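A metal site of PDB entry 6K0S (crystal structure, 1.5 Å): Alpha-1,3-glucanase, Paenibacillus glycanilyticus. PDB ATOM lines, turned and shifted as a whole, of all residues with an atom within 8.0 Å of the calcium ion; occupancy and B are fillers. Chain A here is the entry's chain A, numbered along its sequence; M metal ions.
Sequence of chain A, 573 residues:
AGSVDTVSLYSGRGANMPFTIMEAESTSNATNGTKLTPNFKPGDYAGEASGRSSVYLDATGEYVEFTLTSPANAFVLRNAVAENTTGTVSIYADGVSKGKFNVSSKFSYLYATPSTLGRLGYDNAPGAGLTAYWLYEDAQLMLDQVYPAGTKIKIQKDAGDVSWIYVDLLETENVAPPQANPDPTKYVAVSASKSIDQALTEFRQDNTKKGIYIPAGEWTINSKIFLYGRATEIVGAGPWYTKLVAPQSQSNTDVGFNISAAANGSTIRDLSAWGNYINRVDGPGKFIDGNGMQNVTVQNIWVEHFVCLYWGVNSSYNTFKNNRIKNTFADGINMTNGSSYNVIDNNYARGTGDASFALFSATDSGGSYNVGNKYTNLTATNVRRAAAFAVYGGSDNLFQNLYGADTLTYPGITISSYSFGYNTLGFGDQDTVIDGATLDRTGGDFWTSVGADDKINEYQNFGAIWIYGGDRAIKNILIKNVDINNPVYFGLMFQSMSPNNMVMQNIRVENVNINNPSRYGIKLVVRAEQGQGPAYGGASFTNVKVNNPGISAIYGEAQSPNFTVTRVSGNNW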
ATOM      1  N   ILE A  21       3.835  -1.045  -2.317  1.00  0.00           N
ATOM      2  CA  ILE A  21       5.002  -1.282  -1.449  1.00  0.00           C
ATOM      3  C   ILE A  21       4.497  -1.428  -0.018  1.00  0.00           C
ATOM      4  O   ILE A  21       3.830  -0.526   0.489  1.00  0.00           O
ATOM      5  CB  ILE A  21       6.005  -0.129  -1.533  1.00  0.00           C
ATOM      6  CG1 ILE A  21       6.494   0.094  -2.982  1.00  0.00           C
ATOM      7  CG2 ILE A  21       7.154  -0.363  -0.541  1.00  0.00           C
ATOM      8  CD1 ILE A  21       7.597  -0.821  -3.400  1.00  0.00           C
ATOM      9  N   MET A  22       4.853  -2.530   0.638  1.00  0.00           N
ATOM     10  CA  MET A  22       4.432  -2.779   2.008  1.00  0.00           C
ATOM     11  C   MET A  22       5.649  -3.080   2.874  1.00  0.00           C
ATOM     12  O   MET A  22       6.434  -3.982   2.556  1.00  0.00           O
ATOM     13  CB  MET A  22       3.411  -3.915   2.065  1.00  0.00           C
ATOM     14  CG  MET A  22       2.137  -3.599   1.238  1.00  0.00           C
ATOM     15  SD  MET A  22       0.748  -4.627   1.703  1.00  0.00           S
ATOM     16  CE  MET A  22       1.419  -6.251   1.380  1.00  0.00           C
ATOM     17  N   GLU A  23       5.803  -2.334   3.971  1.00  0.00           N
ATOM     18  CA  GLU A  23       6.949  -2.538   4.845  1.00  0.00           C
ATOM     19  C   GLU A  23       6.726  -3.753   5.732  1.00  0.00           C
ATOM     20  O   GLU A  23       5.648  -3.920   6.311  1.00  0.00           O
ATOM     21  CB  GLU A  23       7.178  -1.303   5.727  1.00  0.00           C
ATOM     22  CG  GLU A  23       7.499  -0.041   4.952  1.00  0.00           C
ATOM     23  CD  GLU A  23       8.883  -0.058   4.312  1.00  0.00           C
ATOM     24  OE1 GLU A  23       9.680  -0.992   4.582  1.00  0.00           O
ATOM     25  OE2 GLU A  23       9.177   0.879   3.545  1.00  0.00           O
ATOM     26  N   ALA A  24       7.752  -4.599   5.826  1.00  0.00           N
ATOM     27  CA  ALA A  24       7.638  -5.803   6.652  1.00  0.00           C
ATOM     28  C   ALA A  24       7.324  -5.457   8.103  1.00  0.00           C
ATOM     29  O   ALA A  24       6.499  -6.124   8.747  1.00  0.00           O
ATOM     30  CB  ALA A  24       8.932  -6.610   6.571  1.00  0.00           C
ATOM     31  N   GLU A  25       7.952  -4.404   8.620  1.00  0.00           N
ATOM     32  CA  GLU A  25       7.907  -4.041  10.038  1.00  0.00           C
ATOM     33  C   GLU A  25       6.630  -3.316  10.448  1.00  0.00           C
ATOM     34  O   GLU A  25       6.526  -2.901  11.611  1.00  0.00           O
ATOM     35  CB  GLU A  25       9.124  -3.166  10.364  1.00  0.00           C
ATOM     36  CG  GLU A  25       9.126  -1.813   9.651  1.00  0.00           C
ATOM     37  CD  GLU A  25       9.833  -1.824   8.292  1.00  0.00           C
ATOM     38  OE1 GLU A  25      10.022  -2.912   7.698  1.00  0.00           O
ATOM     39  OE2 GLU A  25      10.187  -0.725   7.818  1.00  0.00           O
ATOM     40  N   SER A  26       5.676  -3.134   9.533  1.00  0.00           N
ATOM     41  CA  SER A  26       4.428  -2.463   9.880  1.00  0.00           C
ATOM     42  C   SER A  26       3.771  -3.124  11.089  1.00  0.00           C
ATOM     43  O   SER A  26       3.796  -4.350  11.233  1.00  0.00           O
ATOM     44  CB  SER A  26       3.473  -2.490   8.683  1.00  0.00           C
ATOM     45  OG  SER A  26       2.162  -2.075   9.068  1.00  0.00           O
ATOM     46  N   TYR A  45      21.908  -3.243   8.944  1.00  0.00           N
ATOM     47  CA  TYR A  45      20.689  -3.837   8.391  1.00  0.00           C
ATOM     48  C   TYR A  45      19.442  -2.998   8.682  1.00  0.00           C
ATOM     49  O   TYR A  45      18.464  -3.093   7.938  1.00  0.00           O
ATOM     50  CB  TYR A  45      20.508  -5.275   8.895  1.00  0.00           C
ATOM     51  CG  TYR A  45      21.564  -6.195   8.319  1.00  0.00           C
ATOM     52  CD1 TYR A  45      21.547  -6.549   6.968  1.00  0.00           C
ATOM     53  CD2 TYR A  45      22.586  -6.677   9.117  1.00  0.00           C
ATOM     54  CE1 TYR A  45      22.531  -7.378   6.436  1.00  0.00           C
ATOM     55  CE2 TYR A  45      23.575  -7.494   8.604  1.00  0.00           C
ATOM     56  CZ  TYR A  45      23.540  -7.837   7.260  1.00  0.00           C
ATOM     57  OH  TYR A  45      24.548  -8.658   6.771  1.00  0.00           O
ATOM     58  N   ALA A  46      19.455  -2.182   9.739  1.00  0.00           N
ATOM     59  CA  ALA A  46      18.342  -1.245   9.916  1.00  0.00           C
ATOM     60  C   ALA A  46      18.576   0.014   9.096  1.00  0.00           C
ATOM     61  O   ALA A  46      17.697   0.440   8.335  1.00  0.00           O
ATOM     62  CB  ALA A  46      18.166  -0.884  11.394  1.00  0.00           C
ATOM     63  N   GLU A  48      20.044   0.673   6.458  1.00  0.00           N
ATOM     64  CA  GLU A  48      19.952   0.565   5.007  1.00  0.00           C
ATOM     65  C   GLU A  48      18.598   0.062   4.533  1.00  0.00           C
ATOM     66  O   GLU A  48      18.374  -0.028   3.311  1.00  0.00           O
ATOM     67  CB  GLU A  48      21.049  -0.357   4.467  1.00  0.00           C
ATOM     68  CG  GLU A  48      22.440   0.247   4.568  1.00  0.00           C
ATOM     69  CD  GLU A  48      23.446  -0.403   3.643  1.00  0.00           C
ATOM     70  OE1 GLU A  48      23.055  -1.259   2.833  1.00  0.00           O
ATOM     71  OE2 GLU A  48      24.640  -0.035   3.712  1.00  0.00           O
ATOM     72  N   ALA A  49      17.696  -0.275   5.443  1.00  0.00           N
ATOM     73  CA  ALA A  49      16.387  -0.766   5.068  1.00  0.00           C
ATOM     74  C   ALA A  49      15.440   0.374   4.712  1.00  0.00           C
ATOM     75  O   ALA A  49      15.568   1.499   5.198  1.00  0.00           O
ATOM     76  CB  ALA A  49      15.773  -1.590   6.193  1.00  0.00           C
ATOM     77  N   SER A  50      14.464   0.055   3.860  1.00  0.00           N
ATOM     78  CA  SER A  50      13.355   0.965   3.637  1.00  0.00           C
ATOM     79  C   SER A  50      12.612   1.177   4.965  1.00  0.00           C
ATOM     80  O   SER A  50      12.356   0.231   5.713  1.00  0.00           O
ATOM     81  CB  SER A  50      12.429   0.366   2.558  1.00  0.00           C
ATOM     82  OG  SER A  50      11.337   1.224   2.278  1.00  0.00           O
ATOM     83  N   GLY A  51      12.317   2.434   5.284  1.00  0.00           N
ATOM     84  CA  GLY A  51      11.739   2.711   6.591  1.00  0.00           C
ATOM     85  C   GLY A  51      12.715   2.600   7.745  1.00  0.00           C
ATOM     86  O   GLY A  51      12.303   2.746   8.908  1.00  0.00           O
ATOM     87  N   ARG A  52      14.001   2.372   7.453  1.00  0.00           N
ATOM     88  CA  ARG A  52      15.057   2.148   8.448  1.00  0.00           C
ATOM     89  C   ARG A  52      14.749   0.956   9.365  1.00  0.00           C
ATOM     90  O   ARG A  52      15.270   0.874  10.483  1.00  0.00           O
ATOM     91  CB  ARG A  52      15.349   3.412   9.267  1.00  0.00           C
ATOM     92  CG  ARG A  52      15.600   4.643   8.397  1.00  0.00           C
ATOM     93  CD  ARG A  52      16.812   4.524   7.455  1.00  0.00           C
ATOM     94  NE  ARG A  52      16.939   5.753   6.676  1.00  0.00           N
ATOM     95  CZ  ARG A  52      18.097   6.299   6.268  1.00  0.00           C
ATOM     96  NH1 ARG A  52      19.267   5.715   6.534  1.00  0.00           N
ATOM     97  NH2 ARG A  52      18.068   7.454   5.598  1.00  0.00           N
ATOM     98  N   SER A  53      13.988  -0.011   8.879  1.00  0.00           N
ATOM     99  CA  SER A  53      13.734  -1.204   9.663  1.00  0.00           C
ATOM    100  C   SER A  53      13.401  -2.383   8.757  1.00  0.00           C
ATOM    101  O   SER A  53      12.940  -2.222   7.626  1.00  0.00           O
ATOM    102  CB  SER A  53      12.597  -0.961  10.667  1.00  0.00           C
ATOM    103  OG  SER A  53      12.352  -2.111  11.449  1.00  0.00           O
ATOM    104  N   SER A  54      13.646  -3.577   9.295  1.00  0.00           N
ATOM    105  CA  SER A  54      13.298  -4.835   8.654  1.00  0.00           C
ATOM    106  C   SER A  54      12.879  -5.804   9.749  1.00  0.00           C
ATOM    107  O   SER A  54      13.067  -5.537  10.932  1.00  0.00           O
ATOM    108  CB  SER A  54      14.472  -5.419   7.858  1.00  0.00           C
ATOM    109  OG  SER A  54      14.784  -4.628   6.740  1.00  0.00           O
ATOM    110  N   VAL A  55      12.336  -6.951   9.330  1.00  0.00           N
ATOM    111  CA  VAL A  55      12.056  -8.041  10.258  1.00  0.00           C
ATOM    112  C   VAL A  55      13.046  -9.162   9.964  1.00  0.00           C
ATOM    113  O   VAL A  55      13.118  -9.663   8.824  1.00  0.00           O
ATOM    114  CB  VAL A  55      10.609  -8.530  10.188  1.00  0.00           C
ATOM    115  CG1 VAL A  55      10.388  -9.658  11.218  1.00  0.00           C
ATOM    116  CG2 VAL A  55       9.643  -7.364  10.461  1.00  0.00           C
ATOM    117  N   PHE A  66       2.132 -10.362   5.816  1.00  0.00           N
ATOM    118  CA  PHE A  66       1.572  -9.200   5.143  1.00  0.00           C
ATOM    119  C   PHE A  66       0.107  -9.440   4.828  1.00  0.00           C
ATOM    120  O   PHE A  66      -0.356 -10.579   4.745  1.00  0.00           O
ATOM    121  CB  PHE A  66       2.293  -8.903   3.820  1.00  0.00           C
ATOM    122  CG  PHE A  66       3.754  -8.621   3.946  1.00  0.00           C
ATOM    123  CD1 PHE A  66       4.666  -9.651   4.022  1.00  0.00           C
ATOM    124  CD2 PHE A  66       4.215  -7.312   3.950  1.00  0.00           C
ATOM    125  CE1 PHE A  66       6.036  -9.379   4.129  1.00  0.00           C
ATOM    126  CE2 PHE A  66       5.575  -7.043   4.040  1.00  0.00           C
ATOM    127  CZ  PHE A  66       6.481  -8.078   4.121  1.00  0.00           C
ATOM    128  N   ARG A  78      12.323  -7.363  -0.981  1.00  0.00           N
ATOM    129  CA  ARG A  78      13.605  -6.743  -0.686  1.00  0.00           C
ATOM    130  C   ARG A  78      14.103  -7.335   0.612  1.00  0.00           C
ATOM    131  O   ARG A  78      13.377  -7.337   1.616  1.00  0.00           O
ATOM    132  CB  ARG A  78      13.503  -5.222  -0.581  1.00  0.00           C
ATOM    133  CG  ARG A  78      14.883  -4.538  -0.490  1.00  0.00           C
ATOM    134  CD  ARG A  78      14.762  -3.035  -0.497  1.00  0.00           C
ATOM    135  NE  ARG A  78      16.000  -2.360  -0.915  1.00  0.00           N
ATOM    136  CZ  ARG A  78      16.811  -1.683  -0.101  1.00  0.00           C
ATOM    137  NH1 ARG A  78      16.539  -1.590   1.204  1.00  0.00           N
ATOM    138  NH2 ARG A  78      17.897  -1.076  -0.586  1.00  0.00           N
ATOM    139  N   TYR A 136      21.174  -4.862   1.008  1.00  0.00           N
ATOM    140  CA  TYR A 136      19.880  -5.378   0.562  1.00  0.00           C
ATOM    141  C   TYR A 136      19.872  -5.653  -0.937  1.00  0.00           C
ATOM    142  O   TYR A 136      20.597  -5.031  -1.714  1.00  0.00           O
ATOM    143  CB  TYR A 136      18.763  -4.406   0.942  1.00  0.00           C
ATOM    144  CG  TYR A 136      18.421  -4.495   2.400  1.00  0.00           C
ATOM    145  CD1 TYR A 136      17.517  -5.449   2.854  1.00  0.00           C
ATOM    146  CD2 TYR A 136      19.046  -3.686   3.346  1.00  0.00           C
ATOM    147  CE1 TYR A 136      17.225  -5.594   4.193  1.00  0.00           C
ATOM    148  CE2 TYR A 136      18.752  -3.811   4.705  1.00  0.00           C
ATOM    149  CZ  TYR A 136      17.854  -4.778   5.112  1.00  0.00           C
ATOM    150  OH  TYR A 136      17.555  -4.928   6.456  1.00  0.00           O
ATOM    151  N   VAL A 167      13.906  -9.294   6.194  1.00  0.00           N
ATOM    152  CA  VAL A 167      12.815  -8.983   5.270  1.00  0.00           C
ATOM    153  C   VAL A 167      12.464  -7.505   5.426  1.00  0.00           C
ATOM    154  O   VAL A 167      12.009  -7.066   6.486  1.00  0.00           O
ATOM    155  CB  VAL A 167      11.585  -9.860   5.551  1.00  0.00           C
ATOM    156  CG1 VAL A 167      10.444  -9.460   4.613  1.00  0.00           C
ATOM    157  CG2 VAL A 167      11.935 -11.352   5.398  1.00  0.00           C
ATOM    158  N   ASP A 168      12.692  -6.730   4.358  1.00  0.00           N
ATOM    159  CA  ASP A 168      12.569  -5.276   4.418  1.00  0.00           C
ATOM    160  C   ASP A 168      11.204  -4.793   3.966  1.00  0.00           C
ATOM    161  O   ASP A 168      10.498  -4.079   4.705  1.00  0.00           O
ATOM    162  CB  ASP A 168      13.692  -4.654   3.565  1.00  0.00           C
ATOM    163  CG  ASP A 168      13.689  -3.139   3.596  1.00  0.00           C
ATOM    164  OD1 ASP A 168      12.939  -2.564   4.407  1.00  0.00           O
ATOM    165  OD2 ASP A 168      14.435  -2.525   2.797  1.00  0.00           O
ATOM    166  N   LEU A 169      10.798  -5.154   2.757  1.00  0.00           N
ATOM    167  CA  LEU A 169       9.518  -4.754   2.206  1.00  0.00           C
ATOM    168  C   LEU A 169       9.104  -5.798   1.191  1.00  0.00           C
ATOM    169  O   LEU A 169       9.908  -6.618   0.743  1.00  0.00           O
ATOM    170  CB  LEU A 169       9.560  -3.360   1.555  1.00  0.00           C
ATOM    171  CG  LEU A 169      10.510  -3.137   0.354  1.00  0.00           C
ATOM    172  CD1 LEU A 169       9.962  -3.705  -0.981  1.00  0.00           C
ATOM    173  CD2 LEU A 169      10.800  -1.660   0.199  1.00  0.00           C
ATOM    174  N   LEU A 170       7.839  -5.719   0.797  1.00  0.00           N
ATOM    175  CA  LEU A 170       7.266  -6.563  -0.240  1.00  0.00           C
ATOM    176  C   LEU A 170       6.564  -5.660  -1.246  1.00  0.00           C
ATOM    177  O   LEU A 170       5.722  -4.844  -0.858  1.00  0.00           O
ATOM    178  CB  LEU A 170       6.260  -7.555   0.380  1.00  0.00           C
ATOM    179  CG  LEU A 170       5.562  -8.550  -0.549  1.00  0.00           C
ATOM    180  CD1 LEU A 170       6.567  -9.600  -0.991  1.00  0.00           C
ATOM    181  CD2 LEU A 170       4.373  -9.179   0.158  1.00  0.00           C
ATOM    182  N   ASN A 382      15.582   4.506  -1.042  1.00  0.00           N
ATOM    183  CA  ASN A 382      16.755   3.680  -0.777  1.00  0.00           C
ATOM    184  C   ASN A 382      17.914   4.093  -1.690  1.00  0.00           C
ATOM    185  O   ASN A 382      18.480   3.285  -2.426  1.00  0.00           O
ATOM    186  CB  ASN A 382      16.440   2.192  -0.941  1.00  0.00           C
ATOM    187  CG  ASN A 382      15.570   1.647   0.176  1.00  0.00           C
ATOM    188  OD1 ASN A 382      14.500   1.116  -0.089  1.00  0.00           O
ATOM    189  ND2 ASN A 382      16.050   1.737   1.410  1.00  0.00           N
ATOM    190  N   ASP A 406      14.892   7.721   2.453  1.00  0.00           N
ATOM    191  CA  ASP A 406      15.908   6.762   2.886  1.00  0.00           C
ATOM    192  C   ASP A 406      17.183   6.852   2.042  1.00  0.00           C
ATOM    193  O   ASP A 406      17.612   5.901   1.385  1.00  0.00           O
ATOM    194  CB  ASP A 406      15.312   5.343   2.918  1.00  0.00           C
ATOM    195  CG  ASP A 406      14.256   5.203   4.000  1.00  0.00           C
ATOM    196  OD1 ASP A 406      14.511   5.709   5.113  1.00  0.00           O
ATOM    197  OD2 ASP A 406      13.186   4.609   3.747  1.00  0.00           O
ATOM    198  N   ARG A 441      12.998  10.767   5.905  1.00  0.00           N
ATOM    199  CA  ARG A 441      14.274  10.218   6.384  1.00  0.00           C
ATOM    200  C   ARG A 441      15.402  10.423   5.355  1.00  0.00           C
ATOM    201  O   ARG A 441      16.138   9.494   4.999  1.00  0.00           O
ATOM    202  CB  ARG A 441      14.122   8.726   6.743  1.00  0.00           C
ATOM    203  CG  ARG A 441      13.079   8.481   7.849  1.00  0.00           C
ATOM    204  CD  ARG A 441      12.762   6.976   8.059  1.00  0.00           C
ATOM    205  NE  ARG A 441      12.360   6.373   6.790  1.00  0.00           N
ATOM    206  CZ  ARG A 441      11.130   6.394   6.297  1.00  0.00           C
ATOM    207  NH1 ARG A 441      10.142   6.952   6.976  1.00  0.00           N
ATOM    208  NH2 ARG A 441      10.896   5.843   5.101  1.00  0.00           N
HETATM  209 CA    CA M   1      11.324  -1.921   5.892  1.00  0.00          CA
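OD1 of Asp 168 binds the calcium ion (2.3 Å).
The calcium ion is bound by OE1 of Glu 23 (2.3 Å).
The calcium ion is bound by O of Ser 53.
The calcium ion is bound by O of Ser 50, 2.4 Å away.
The side-chain carboxylate (OE1) of Glu 25 binds the calcium ion, at 2.4 Å.
OE2 of Glu 25 binds the calcium ion, 2.5 Å away.
The backbone carbonyl oxygen (O) of Asp 168 binds the calcium ion, at 2.6 Å.
The nearest printed residue that does not touch the calcium ion is Ser 54 (4.4 Å).
O of Asp 168 lies close to N of Ala 24, at 3.0 Å.
OD2 of Asp 168 is in salt-bridge range of NH1 of Arg 78 (2.8 Å).
The backbone NH of Ser 50 sits close to the side-chain amide nitrogen of Asn 382, at 3.4 Å.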
